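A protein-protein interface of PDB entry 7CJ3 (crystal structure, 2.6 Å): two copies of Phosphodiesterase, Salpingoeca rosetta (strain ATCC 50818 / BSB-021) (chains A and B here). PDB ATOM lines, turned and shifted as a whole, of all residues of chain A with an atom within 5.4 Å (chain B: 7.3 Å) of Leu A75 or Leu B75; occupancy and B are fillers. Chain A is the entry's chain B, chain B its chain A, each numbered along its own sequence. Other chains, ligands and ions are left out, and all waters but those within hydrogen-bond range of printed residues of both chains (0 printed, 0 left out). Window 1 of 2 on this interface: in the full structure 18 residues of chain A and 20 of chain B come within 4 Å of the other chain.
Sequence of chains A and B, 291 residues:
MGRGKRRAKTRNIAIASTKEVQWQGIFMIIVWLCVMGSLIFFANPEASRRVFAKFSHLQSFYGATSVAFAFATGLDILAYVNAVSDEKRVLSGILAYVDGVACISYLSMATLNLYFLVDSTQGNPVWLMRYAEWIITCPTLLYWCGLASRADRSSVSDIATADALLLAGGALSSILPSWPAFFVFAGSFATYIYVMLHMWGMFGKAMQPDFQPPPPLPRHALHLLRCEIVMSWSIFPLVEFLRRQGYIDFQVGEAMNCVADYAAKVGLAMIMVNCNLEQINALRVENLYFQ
Among the printed residues, merely in contact across the chains: Phe A71 with Val B266 (3.9 Å), Gly A74 with Met B270 (3.96 Å), Leu A75 with Leu B75 (3.5 Å), Leu A75 with Val B273 (3.6 Å), Leu A78 with Met B270 (3.2 Å), Met A270 with Leu B78 (3.4 Å) and Val A273 with Leu B75 (3.9 Å).
Leu A75 touches just these residues of chain B: Leu B75 and Val B273.
Of chain A, only Leu A75 (3.5 Å) and Val A273 (3.9 Å) come within 4 Å of Leu B75.
Of the printed residues of chain B, Met A270 touches Leu B78.
Of the printed residues of chain B, Leu A78 touches Met B270 (3.2 Å) and Asn B274 (3.5 Å).
Of the printed residues of chain A, Met B270 touches Phe A71 (3.8 Å), Gly A74 (3.96 Å) and Leu A78 (3.2 Å).
Of the printed residues of chain A, Asn B274 touches Leu A78.
Printed residues of chain A within 4 Å of Val B266: Phe A71 (3.9 Å).
The nearest printed residue of chain A that does not touch Leu B78 is Val A273 (5.7 Å).
Phe A71 touches Met B270, but with the chains exchanged Met A270 does not touch Phe B71 (4.03 Å).
Gly A74 touches Met B270, but with the chains exchanged Met A270 does not touch Gly B74 (4.3 Å).
Leu A75 touches its own counterpart, Leu B75.
Leu A75 touches Val B273, and with the chains exchanged Val A273 touches Leu B75.
Positions printed for both chains: 70, 71, 72, 73, 74, 75, 76, 77, 78, 79, 269, 270 and 273.
Of the 9 pairs that touch across the chains among the printed residues, 5 have their exchanged pair printed and touching as well.
Printed residues of chain A that touch a printed residue of chain B: Phe A71, Gly A74, Leu A75, Leu A78, Met A270 and Val A273.
Hydrophobic or aromatic side chains of chain A that line the printed part of chain B: Phe A71, Leu A75, Leu A78 and Val A273.
Among the printed residues, no Asp or Glu carboxylate lies within 4 Å of a Lys or Arg side-chain nitrogen of the other chain.
The backbone carbonyl oxygen (O) of Leu A78 sits close to the side-chain amide oxygen (OD1) of Asn B274 (3.5 Å).
O of Phe A71 lies close to SD of Met B270 (3.8 Å).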
ATOM      1  N   ALA A  70      21.246   6.176  -3.128  1.00  0.00           N
ATOM      2  CA  ALA A  70      21.778   6.394  -4.488  1.00  0.00           C
ATOM      3  C   ALA A  70      22.851   7.494  -4.438  1.00  0.00           C
ATOM      4  O   ALA A  70      23.994   7.218  -4.869  1.00  0.00           O
ATOM      5  CB  ALA A  70      20.659   6.711  -5.453  1.00  0.00           C
ATOM      6  N   PHE A  71      22.508   8.682  -3.922  1.00  0.00           N
ATOM      7  CA  PHE A  71      23.437   9.839  -3.761  1.00  0.00           C
ATOM      8  C   PHE A  71      24.587   9.472  -2.820  1.00  0.00           C
ATOM      9  O   PHE A  71      25.731   9.890  -3.118  1.00  0.00           O
ATOM     10  CB  PHE A  71      22.703  11.109  -3.308  1.00  0.00           C
ATOM     11  CG  PHE A  71      21.992  11.810  -4.447  1.00  0.00           C
ATOM     12  CD1 PHE A  71      22.693  12.583  -5.359  1.00  0.00           C
ATOM     13  CD2 PHE A  71      20.631  11.644  -4.641  1.00  0.00           C
ATOM     14  CE1 PHE A  71      22.045  13.157  -6.436  1.00  0.00           C
ATOM     15  CE2 PHE A  71      19.989  12.217  -5.722  1.00  0.00           C
ATOM     16  CZ  PHE A  71      20.695  12.982  -6.618  1.00  0.00           C
ATOM     17  N   ALA A  72      24.299   8.718  -1.741  1.00  0.00           N
ATOM     18  CA  ALA A  72      25.320   8.206  -0.797  1.00  0.00           C
ATOM     19  C   ALA A  72      26.329   7.346  -1.553  1.00  0.00           C
ATOM     20  O   ALA A  72      27.526   7.465  -1.245  1.00  0.00           O
ATOM     21  CB  ALA A  72      24.696   7.431   0.322  1.00  0.00           C
ATOM     22  N   THR A  73      25.863   6.509  -2.483  1.00  0.00           N
ATOM     23  CA  THR A  73      26.702   5.599  -3.314  1.00  0.00           C
ATOM     24  C   THR A  73      27.525   6.432  -4.312  1.00  0.00           C
ATOM     25  O   THR A  73      28.720   6.138  -4.517  1.00  0.00           O
ATOM     26  CB  THR A  73      25.853   4.531  -4.009  1.00  0.00           C
ATOM     27  OG1 THR A  73      24.940   3.941  -3.088  1.00  0.00           O
ATOM     28  CG2 THR A  73      26.702   3.435  -4.599  1.00  0.00           C
ATOM     29  N   GLY A  74      26.912   7.456  -4.892  1.00  0.00           N
ATOM     30  CA  GLY A  74      27.610   8.473  -5.702  1.00  0.00           C
ATOM     31  C   GLY A  74      28.855   8.982  -5.001  1.00  0.00           C
ATOM     32  O   GLY A  74      29.941   8.926  -5.607  1.00  0.00           O
ATOM     33  N   LEU A  75      28.708   9.448  -3.758  1.00  0.00           N
ATOM     34  CA  LEU A  75      29.799  10.077  -2.966  1.00  0.00           C
ATOM     35  C   LEU A  75      30.915   9.062  -2.701  1.00  0.00           C
ATOM     36  O   LEU A  75      32.096   9.460  -2.758  1.00  0.00           O
ATOM     37  CB  LEU A  75      29.223  10.608  -1.655  1.00  0.00           C
ATOM     38  CG  LEU A  75      30.231  11.247  -0.699  1.00  0.00           C
ATOM     39  CD1 LEU A  75      30.983  12.387  -1.368  1.00  0.00           C
ATOM     40  CD2 LEU A  75      29.533  11.729   0.563  1.00  0.00           C
ATOM     41  N   ASP A  76      30.561   7.811  -2.401  1.00  0.00           N
ATOM     42  CA  ASP A  76      31.543   6.735  -2.107  1.00  0.00           C
ATOM     43  C   ASP A  76      32.358   6.419  -3.367  1.00  0.00           C
ATOM     44  O   ASP A  76      33.536   6.078  -3.212  1.00  0.00           O
ATOM     45  CB  ASP A  76      30.857   5.474  -1.593  1.00  0.00           C
ATOM     46  CG  ASP A  76      30.285   5.620  -0.198  1.00  0.00           C
ATOM     47  OD1 ASP A  76      31.067   5.755   0.760  1.00  0.00           O
ATOM     48  OD2 ASP A  76      29.062   5.583  -0.088  1.00  0.00           O
ATOM     49  N   ILE A  77      31.746   6.476  -4.558  1.00  0.00           N
ATOM     50  CA  ILE A  77      32.444   6.174  -5.840  1.00  0.00           C
ATOM     51  C   ILE A  77      33.552   7.221  -5.997  1.00  0.00           C
ATOM     52  O   ILE A  77      34.691   6.833  -6.305  1.00  0.00           O
ATOM     53  CB  ILE A  77      31.471   6.138  -7.047  1.00  0.00           C
ATOM     54  CG1 ILE A  77      30.576   4.889  -7.043  1.00  0.00           C
ATOM     55  CG2 ILE A  77      32.217   6.290  -8.369  1.00  0.00           C
ATOM     56  CD1 ILE A  77      29.276   5.050  -7.827  1.00  0.00           C
ATOM     57  N   LEU A  78      33.235   8.500  -5.756  1.00  0.00           N
ATOM     58  CA  LEU A  78      34.190   9.623  -5.947  1.00  0.00           C
ATOM     59  C   LEU A  78      35.342   9.464  -4.951  1.00  0.00           C
ATOM     60  O   LEU A  78      36.461   9.845  -5.291  1.00  0.00           O
ATOM     61  CB  LEU A  78      33.478  10.968  -5.789  1.00  0.00           C
ATOM     62  CG  LEU A  78      32.347  11.242  -6.781  1.00  0.00           C
ATOM     63  CD1 LEU A  78      31.890  12.704  -6.715  1.00  0.00           C
ATOM     64  CD2 LEU A  78      32.766  10.877  -8.196  1.00  0.00           C
ATOM     65  N   ALA A  79      35.084   8.896  -3.776  1.00  0.00           N
ATOM     66  CA  ALA A  79      36.104   8.618  -2.740  1.00  0.00           C
ATOM     67  C   ALA A  79      37.008   7.463  -3.187  1.00  0.00           C
ATOM     68  O   ALA A  79      38.190   7.466  -2.787  1.00  0.00           O
ATOM     69  CB  ALA A  79      35.433   8.311  -1.419  1.00  0.00           C
ATOM     70  N   ALA A 269      30.798   7.110   5.980  1.00  0.00           N
ATOM     71  CA  ALA A 269      31.327   7.785   4.774  1.00  0.00           C
ATOM     72  C   ALA A 269      31.608   9.248   5.064  1.00  0.00           C
ATOM     73  O   ALA A 269      32.494   9.777   4.420  1.00  0.00           O
ATOM     74  CB  ALA A 269      30.370   7.660   3.624  1.00  0.00           C
ATOM     75  N   MET A 270      30.859   9.885   5.958  1.00  0.00           N
ATOM     76  CA  MET A 270      31.125  11.290   6.378  1.00  0.00           C
ATOM     77  C   MET A 270      32.441  11.346   7.173  1.00  0.00           C
ATOM     78  O   MET A 270      33.208  12.296   6.957  1.00  0.00           O
ATOM     79  CB  MET A 270      29.969  11.860   7.207  1.00  0.00           C
ATOM     80  CG  MET A 270      28.805  12.370   6.375  1.00  0.00           C
ATOM     81  SD  MET A 270      27.245  12.667   7.321  1.00  0.00           S
ATOM     82  CE  MET A 270      27.774  13.502   8.822  1.00  0.00           C
ATOM     83  N   VAL A 273      35.573  10.650   4.754  1.00  0.00           N
ATOM     84  CA  VAL A 273      35.751  11.878   3.917  1.00  0.00           C
ATOM     85  C   VAL A 273      36.689  12.867   4.639  1.00  0.00           C
ATOM     86  O   VAL A 273      37.536  13.482   3.971  1.00  0.00           O
ATOM     87  CB  VAL A 273      34.391  12.531   3.604  1.00  0.00           C
ATOM     88  CG1 VAL A 273      34.527  13.996   3.189  1.00  0.00           C
ATOM     89  CG2 VAL A 273      33.616  11.739   2.564  1.00  0.00           C
ATOM     90  N   PHE B  69      18.847  17.028   3.708  1.00  0.00           N
ATOM     91  CA  PHE B  69      19.649  18.280   3.802  1.00  0.00           C
ATOM     92  C   PHE B  69      20.407  18.400   5.138  1.00  0.00           C
ATOM     93  O   PHE B  69      21.535  18.873   5.158  1.00  0.00           O
ATOM     94  CB  PHE B  69      18.748  19.478   3.574  1.00  0.00           C
ATOM     95  CG  PHE B  69      18.536  19.757   2.117  1.00  0.00           C
ATOM     96  CD1 PHE B  69      19.577  20.247   1.348  1.00  0.00           C
ATOM     97  CD2 PHE B  69      17.312  19.534   1.516  1.00  0.00           C
ATOM     98  CE1 PHE B  69      19.383  20.548   0.014  1.00  0.00           C
ATOM     99  CE2 PHE B  69      17.118  19.829   0.181  1.00  0.00           C
ATOM    100  CZ  PHE B  69      18.146  20.353  -0.554  1.00  0.00           C
ATOM    101  N   ALA B  70      19.809  18.001   6.251  1.00  0.00           N
ATOM    102  CA  ALA B  70      20.506  17.979   7.557  1.00  0.00           C
ATOM    103  C   ALA B  70      21.840  17.238   7.398  1.00  0.00           C
ATOM    104  O   ALA B  70      22.883  17.846   7.720  1.00  0.00           O
ATOM    105  CB  ALA B  70      19.618  17.377   8.623  1.00  0.00           C
ATOM    106  N   PHE B  71      21.811  15.985   6.910  1.00  0.00           N
ATOM    107  CA  PHE B  71      23.021  15.149   6.658  1.00  0.00           C
ATOM    108  C   PHE B  71      23.921  15.818   5.611  1.00  0.00           C
ATOM    109  O   PHE B  71      25.164  15.762   5.805  1.00  0.00           O
ATOM    110  CB  PHE B  71      22.657  13.716   6.252  1.00  0.00           C
ATOM    111  CG  PHE B  71      22.284  12.843   7.422  1.00  0.00           C
ATOM    112  CD1 PHE B  71      23.263  12.302   8.230  1.00  0.00           C
ATOM    113  CD2 PHE B  71      20.960  12.602   7.743  1.00  0.00           C
ATOM    114  CE1 PHE B  71      22.922  11.541   9.340  1.00  0.00           C
ATOM    115  CE2 PHE B  71      20.621  11.796   8.814  1.00  0.00           C
ATOM    116  CZ  PHE B  71      21.604  11.294   9.633  1.00  0.00           C
ATOM    117  N   ALA B  72      23.328  16.430   4.566  1.00  0.00           N
ATOM    118  CA  ALA B  72      24.064  17.194   3.538  1.00  0.00           C
ATOM    119  C   ALA B  72      24.843  18.330   4.199  1.00  0.00           C
ATOM    120  O   ALA B  72      25.994  18.555   3.782  1.00  0.00           O
ATOM    121  CB  ALA B  72      23.141  17.730   2.486  1.00  0.00           C
ATOM    122  N   THR B  73      24.237  19.016   5.169  1.00  0.00           N
ATOM    123  CA  THR B  73      24.844  20.151   5.924  1.00  0.00           C
ATOM    124  C   THR B  73      25.963  19.621   6.838  1.00  0.00           C
ATOM    125  O   THR B  73      27.031  20.258   6.927  1.00  0.00           O
ATOM    126  CB  THR B  73      23.785  20.939   6.705  1.00  0.00           C
ATOM    127  OG1 THR B  73      22.664  21.215   5.868  1.00  0.00           O
ATOM    128  CG2 THR B  73      24.324  22.250   7.213  1.00  0.00           C
ATOM    129  N   GLY B  74      25.730  18.475   7.470  1.00  0.00           N
ATOM    130  CA  GLY B  74      26.766  17.733   8.212  1.00  0.00           C
ATOM    131  C   GLY B  74      28.037  17.590   7.398  1.00  0.00           C
ATOM    132  O   GLY B  74      29.107  17.973   7.900  1.00  0.00           O
ATOM    133  N   LEU B  75      27.922  17.070   6.174  1.00  0.00           N
ATOM    134  CA  LEU B  75      29.075  16.767   5.284  1.00  0.00           C
ATOM    135  C   LEU B  75      29.819  18.051   4.918  1.00  0.00           C
ATOM    136  O   LEU B  75      31.066  18.016   4.864  1.00  0.00           O
ATOM    137  CB  LEU B  75      28.568  16.053   4.029  1.00  0.00           C
ATOM    138  CG  LEU B  75      29.641  15.690   3.008  1.00  0.00           C
ATOM    139  CD1 LEU B  75      30.749  14.834   3.633  1.00  0.00           C
ATOM    140  CD2 LEU B  75      29.018  14.989   1.809  1.00  0.00           C
ATOM    141  N   ASP B  76      29.089  19.135   4.650  1.00  0.00           N
ATOM    142  CA  ASP B  76      29.684  20.443   4.268  1.00  0.00           C
ATOM    143  C   ASP B  76      30.478  21.017   5.450  1.00  0.00           C
ATOM    144  O   ASP B  76      31.484  21.682   5.188  1.00  0.00           O
ATOM    145  CB  ASP B  76      28.617  21.438   3.817  1.00  0.00           C
ATOM    146  CG  ASP B  76      27.992  21.095   2.486  1.00  0.00           C
ATOM    147  OD1 ASP B  76      28.702  21.175   1.458  1.00  0.00           O
ATOM    148  OD2 ASP B  76      26.806  20.772   2.494  1.00  0.00           O
ATOM    149  N   ILE B  77      30.016  20.816   6.688  1.00  0.00           N
ATOM    150  CA  ILE B  77      30.705  21.339   7.905  1.00  0.00           C
ATOM    151  C   ILE B  77      32.080  20.662   7.960  1.00  0.00           C
ATOM    152  O   ILE B  77      33.075  21.370   8.165  1.00  0.00           O
ATOM    153  CB  ILE B  77      29.871  21.124   9.195  1.00  0.00           C
ATOM    154  CG1 ILE B  77      28.657  22.059   9.270  1.00  0.00           C
ATOM    155  CG2 ILE B  77      30.738  21.258  10.434  1.00  0.00           C
ATOM    156  CD1 ILE B  77      27.528  21.573  10.163  1.00  0.00           C
ATOM    157  N   LEU B  78      32.131  19.347   7.748  1.00  0.00           N
ATOM    158  CA  LEU B  78      33.387  18.551   7.846  1.00  0.00           C
ATOM    159  C   LEU B  78      34.351  19.016   6.748  1.00  0.00           C
ATOM    160  O   LEU B  78      35.558  18.990   6.987  1.00  0.00           O
ATOM    161  CB  LEU B  78      33.091  17.051   7.750  1.00  0.00           C
ATOM    162  CG  LEU B  78      32.955  16.317   9.084  1.00  0.00           C
ATOM    163  CD1 LEU B  78      32.087  17.089  10.056  1.00  0.00           C
ATOM    164  CD2 LEU B  78      32.389  14.910   8.901  1.00  0.00           C
ATOM    165  N   ALA B  79      33.833  19.454   5.604  1.00  0.00           N
ATOM    166  CA  ALA B  79      34.632  19.995   4.481  1.00  0.00           C
ATOM    167  C   ALA B  79      35.196  21.376   4.849  1.00  0.00           C
ATOM    168  O   ALA B  79      36.281  21.713   4.344  1.00  0.00           O
ATOM    169  CB  ALA B  79      33.789  20.058   3.227  1.00  0.00           C
ATOM    170  N   TYR B  80      34.484  22.151   5.673  1.00  0.00           N
ATOM    171  CA  TYR B  80      34.875  23.525   6.089  1.00  0.00           C
ATOM    172  C   TYR B  80      35.984  23.452   7.145  1.00  0.00           C
ATOM    173  O   TYR B  80      37.026  24.126   6.974  1.00  0.00           O
ATOM    174  CB  TYR B  80      33.682  24.310   6.643  1.00  0.00           C
ATOM    175  CG  TYR B  80      33.992  25.744   6.992  1.00  0.00           C
ATOM    176  CD1 TYR B  80      34.431  26.089   8.261  1.00  0.00           C
ATOM    177  CD2 TYR B  80      33.817  26.765   6.072  1.00  0.00           C
ATOM    178  CE1 TYR B  80      34.715  27.402   8.599  1.00  0.00           C
ATOM    179  CE2 TYR B  80      34.088  28.084   6.397  1.00  0.00           C
ATOM    180  CZ  TYR B  80      34.537  28.404   7.665  1.00  0.00           C
ATOM    181  OH  TYR B  80      34.798  29.707   7.991  1.00  0.00           O
ATOM    182  N   SER B  92      33.208  25.518   0.688  1.00  0.00           N
ATOM    183  CA  SER B  92      32.481  24.496   1.479  1.00  0.00           C
ATOM    184  C   SER B  92      31.589  25.175   2.514  1.00  0.00           C
ATOM    185  O   SER B  92      30.567  24.560   2.885  1.00  0.00           O
ATOM    186  CB  SER B  92      33.418  23.511   2.114  1.00  0.00           C
ATOM    187  OG  SER B  92      33.621  22.410   1.247  1.00  0.00           O
ATOM    188  N   ALA B  96      27.332  24.912   3.099  1.00  0.00           N
ATOM    189  CA  ALA B  96      26.798  24.596   4.441  1.00  0.00           C
ATOM    190  C   ALA B  96      25.544  25.439   4.726  1.00  0.00           C
ATOM    191  O   ALA B  96      24.565  24.837   5.177  1.00  0.00           O
ATOM    192  CB  ALA B  96      27.879  24.793   5.465  1.00  0.00           C
ATOM    193  N   ASP B  99      22.543  24.603   2.249  1.00  0.00           N
ATOM    194  CA  ASP B  99      21.979  23.276   2.601  1.00  0.00           C
ATOM    195  C   ASP B  99      21.199  23.371   3.913  1.00  0.00           C
ATOM    196  O   ASP B  99      20.145  22.739   4.028  1.00  0.00           O
ATOM    197  CB  ASP B  99      23.087  22.219   2.656  1.00  0.00           C
ATOM    198  CG  ASP B  99      23.473  21.724   1.273  1.00  0.00           C
ATOM    199  OD1 ASP B  99      22.870  22.174   0.295  1.00  0.00           O
ATOM    200  OD2 ASP B  99      24.347  20.881   1.183  1.00  0.00           O
ATOM    201  N   VAL B 266      23.318  18.941  -3.384  1.00  0.00           N
ATOM    202  CA  VAL B 266      24.349  17.977  -2.887  1.00  0.00           C
ATOM    203  C   VAL B 266      25.265  17.565  -4.040  1.00  0.00           C
ATOM    204  O   VAL B 266      26.416  17.127  -3.777  1.00  0.00           O
ATOM    205  CB  VAL B 266      23.731  16.742  -2.228  1.00  0.00           C
ATOM    206  CG1 VAL B 266      22.849  17.142  -1.052  1.00  0.00           C
ATOM    207  CG2 VAL B 266      22.977  15.910  -3.252  1.00  0.00           C
ATOM    208  N   ALA B 269      28.382  19.664  -3.694  1.00  0.00           N
ATOM    209  CA  ALA B 269      29.191  19.200  -2.544  1.00  0.00           C
ATOM    210  C   ALA B 269      29.857  17.868  -2.872  1.00  0.00           C
ATOM    211  O   ALA B 269      30.915  17.628  -2.321  1.00  0.00           O
ATOM    212  CB  ALA B 269      28.350  19.055  -1.310  1.00  0.00           C
ATOM    213  N   MET B 270      29.247  17.029  -3.700  1.00  0.00           N
ATOM    214  CA  MET B 270      29.868  15.754  -4.156  1.00  0.00           C
ATOM    215  C   MET B 270      31.061  16.063  -5.074  1.00  0.00           C
ATOM    216  O   MET B 270      32.079  15.379  -4.949  1.00  0.00           O
ATOM    217  CB  MET B 270      28.850  14.856  -4.873  1.00  0.00           C
ATOM    218  CG  MET B 270      27.982  14.046  -3.899  1.00  0.00           C
ATOM    219  SD  MET B 270      26.493  13.266  -4.635  1.00  0.00           S
ATOM    220  CE  MET B 270      27.185  12.417  -6.058  1.00  0.00           C
ATOM    221  N   ILE B 271      30.953  17.060  -5.952  1.00  0.00           N
ATOM    222  CA  ILE B 271      31.982  17.374  -6.997  1.00  0.00           C
ATOM    223  C   ILE B 271      33.202  18.036  -6.326  1.00  0.00           C
ATOM    224  O   ILE B 271      34.346  17.774  -6.768  1.00  0.00           O
ATOM    225  CB  ILE B 271      31.380  18.217  -8.155  1.00  0.00           C
ATOM    226  CG1 ILE B 271      30.537  17.344  -9.098  1.00  0.00           C
ATOM    227  CG2 ILE B 271      32.452  18.988  -8.921  1.00  0.00           C
ATOM    228  CD1 ILE B 271      29.538  18.104  -9.949  1.00  0.00           C
ATOM    229  N   VAL B 273      34.072  17.657  -2.955  1.00  0.00           N
ATOM    230  CA  VAL B 273      34.669  16.538  -2.154  1.00  0.00           C
ATOM    231  C   VAL B 273      35.772  15.845  -2.977  1.00  0.00           C
ATOM    232  O   VAL B 273      36.811  15.500  -2.403  1.00  0.00           O
ATOM    233  CB  VAL B 273      33.581  15.533  -1.724  1.00  0.00           C
ATOM    234  CG1 VAL B 273      34.159  14.171  -1.351  1.00  0.00           C
ATOM    235  CG2 VAL B 273      32.721  16.096  -0.600  1.00  0.00           C
ATOM    236  N   ASN B 274      35.531  15.643  -4.274  1.00  0.00           N
ATOM    237  CA  ASN B 274      36.447  14.979  -5.234  1.00  0.00           C
ATOM    238  C   ASN B 274      37.678  15.860  -5.480  1.00  0.00           C
ATOM    239  O   ASN B 274      38.789  15.299  -5.535  1.00  0.00           O
ATOM    240  CB  ASN B 274      35.730  14.674  -6.551  1.00  0.00           C
ATOM    241  CG  ASN B 274      36.564  13.845  -7.506  1.00  0.00           C
ATOM    242  OD1 ASN B 274      36.628  12.629  -7.379  1.00  0.00           O
ATOM    243  ND2 ASN B 274      37.220  14.490  -8.458  1.00  0.00           N
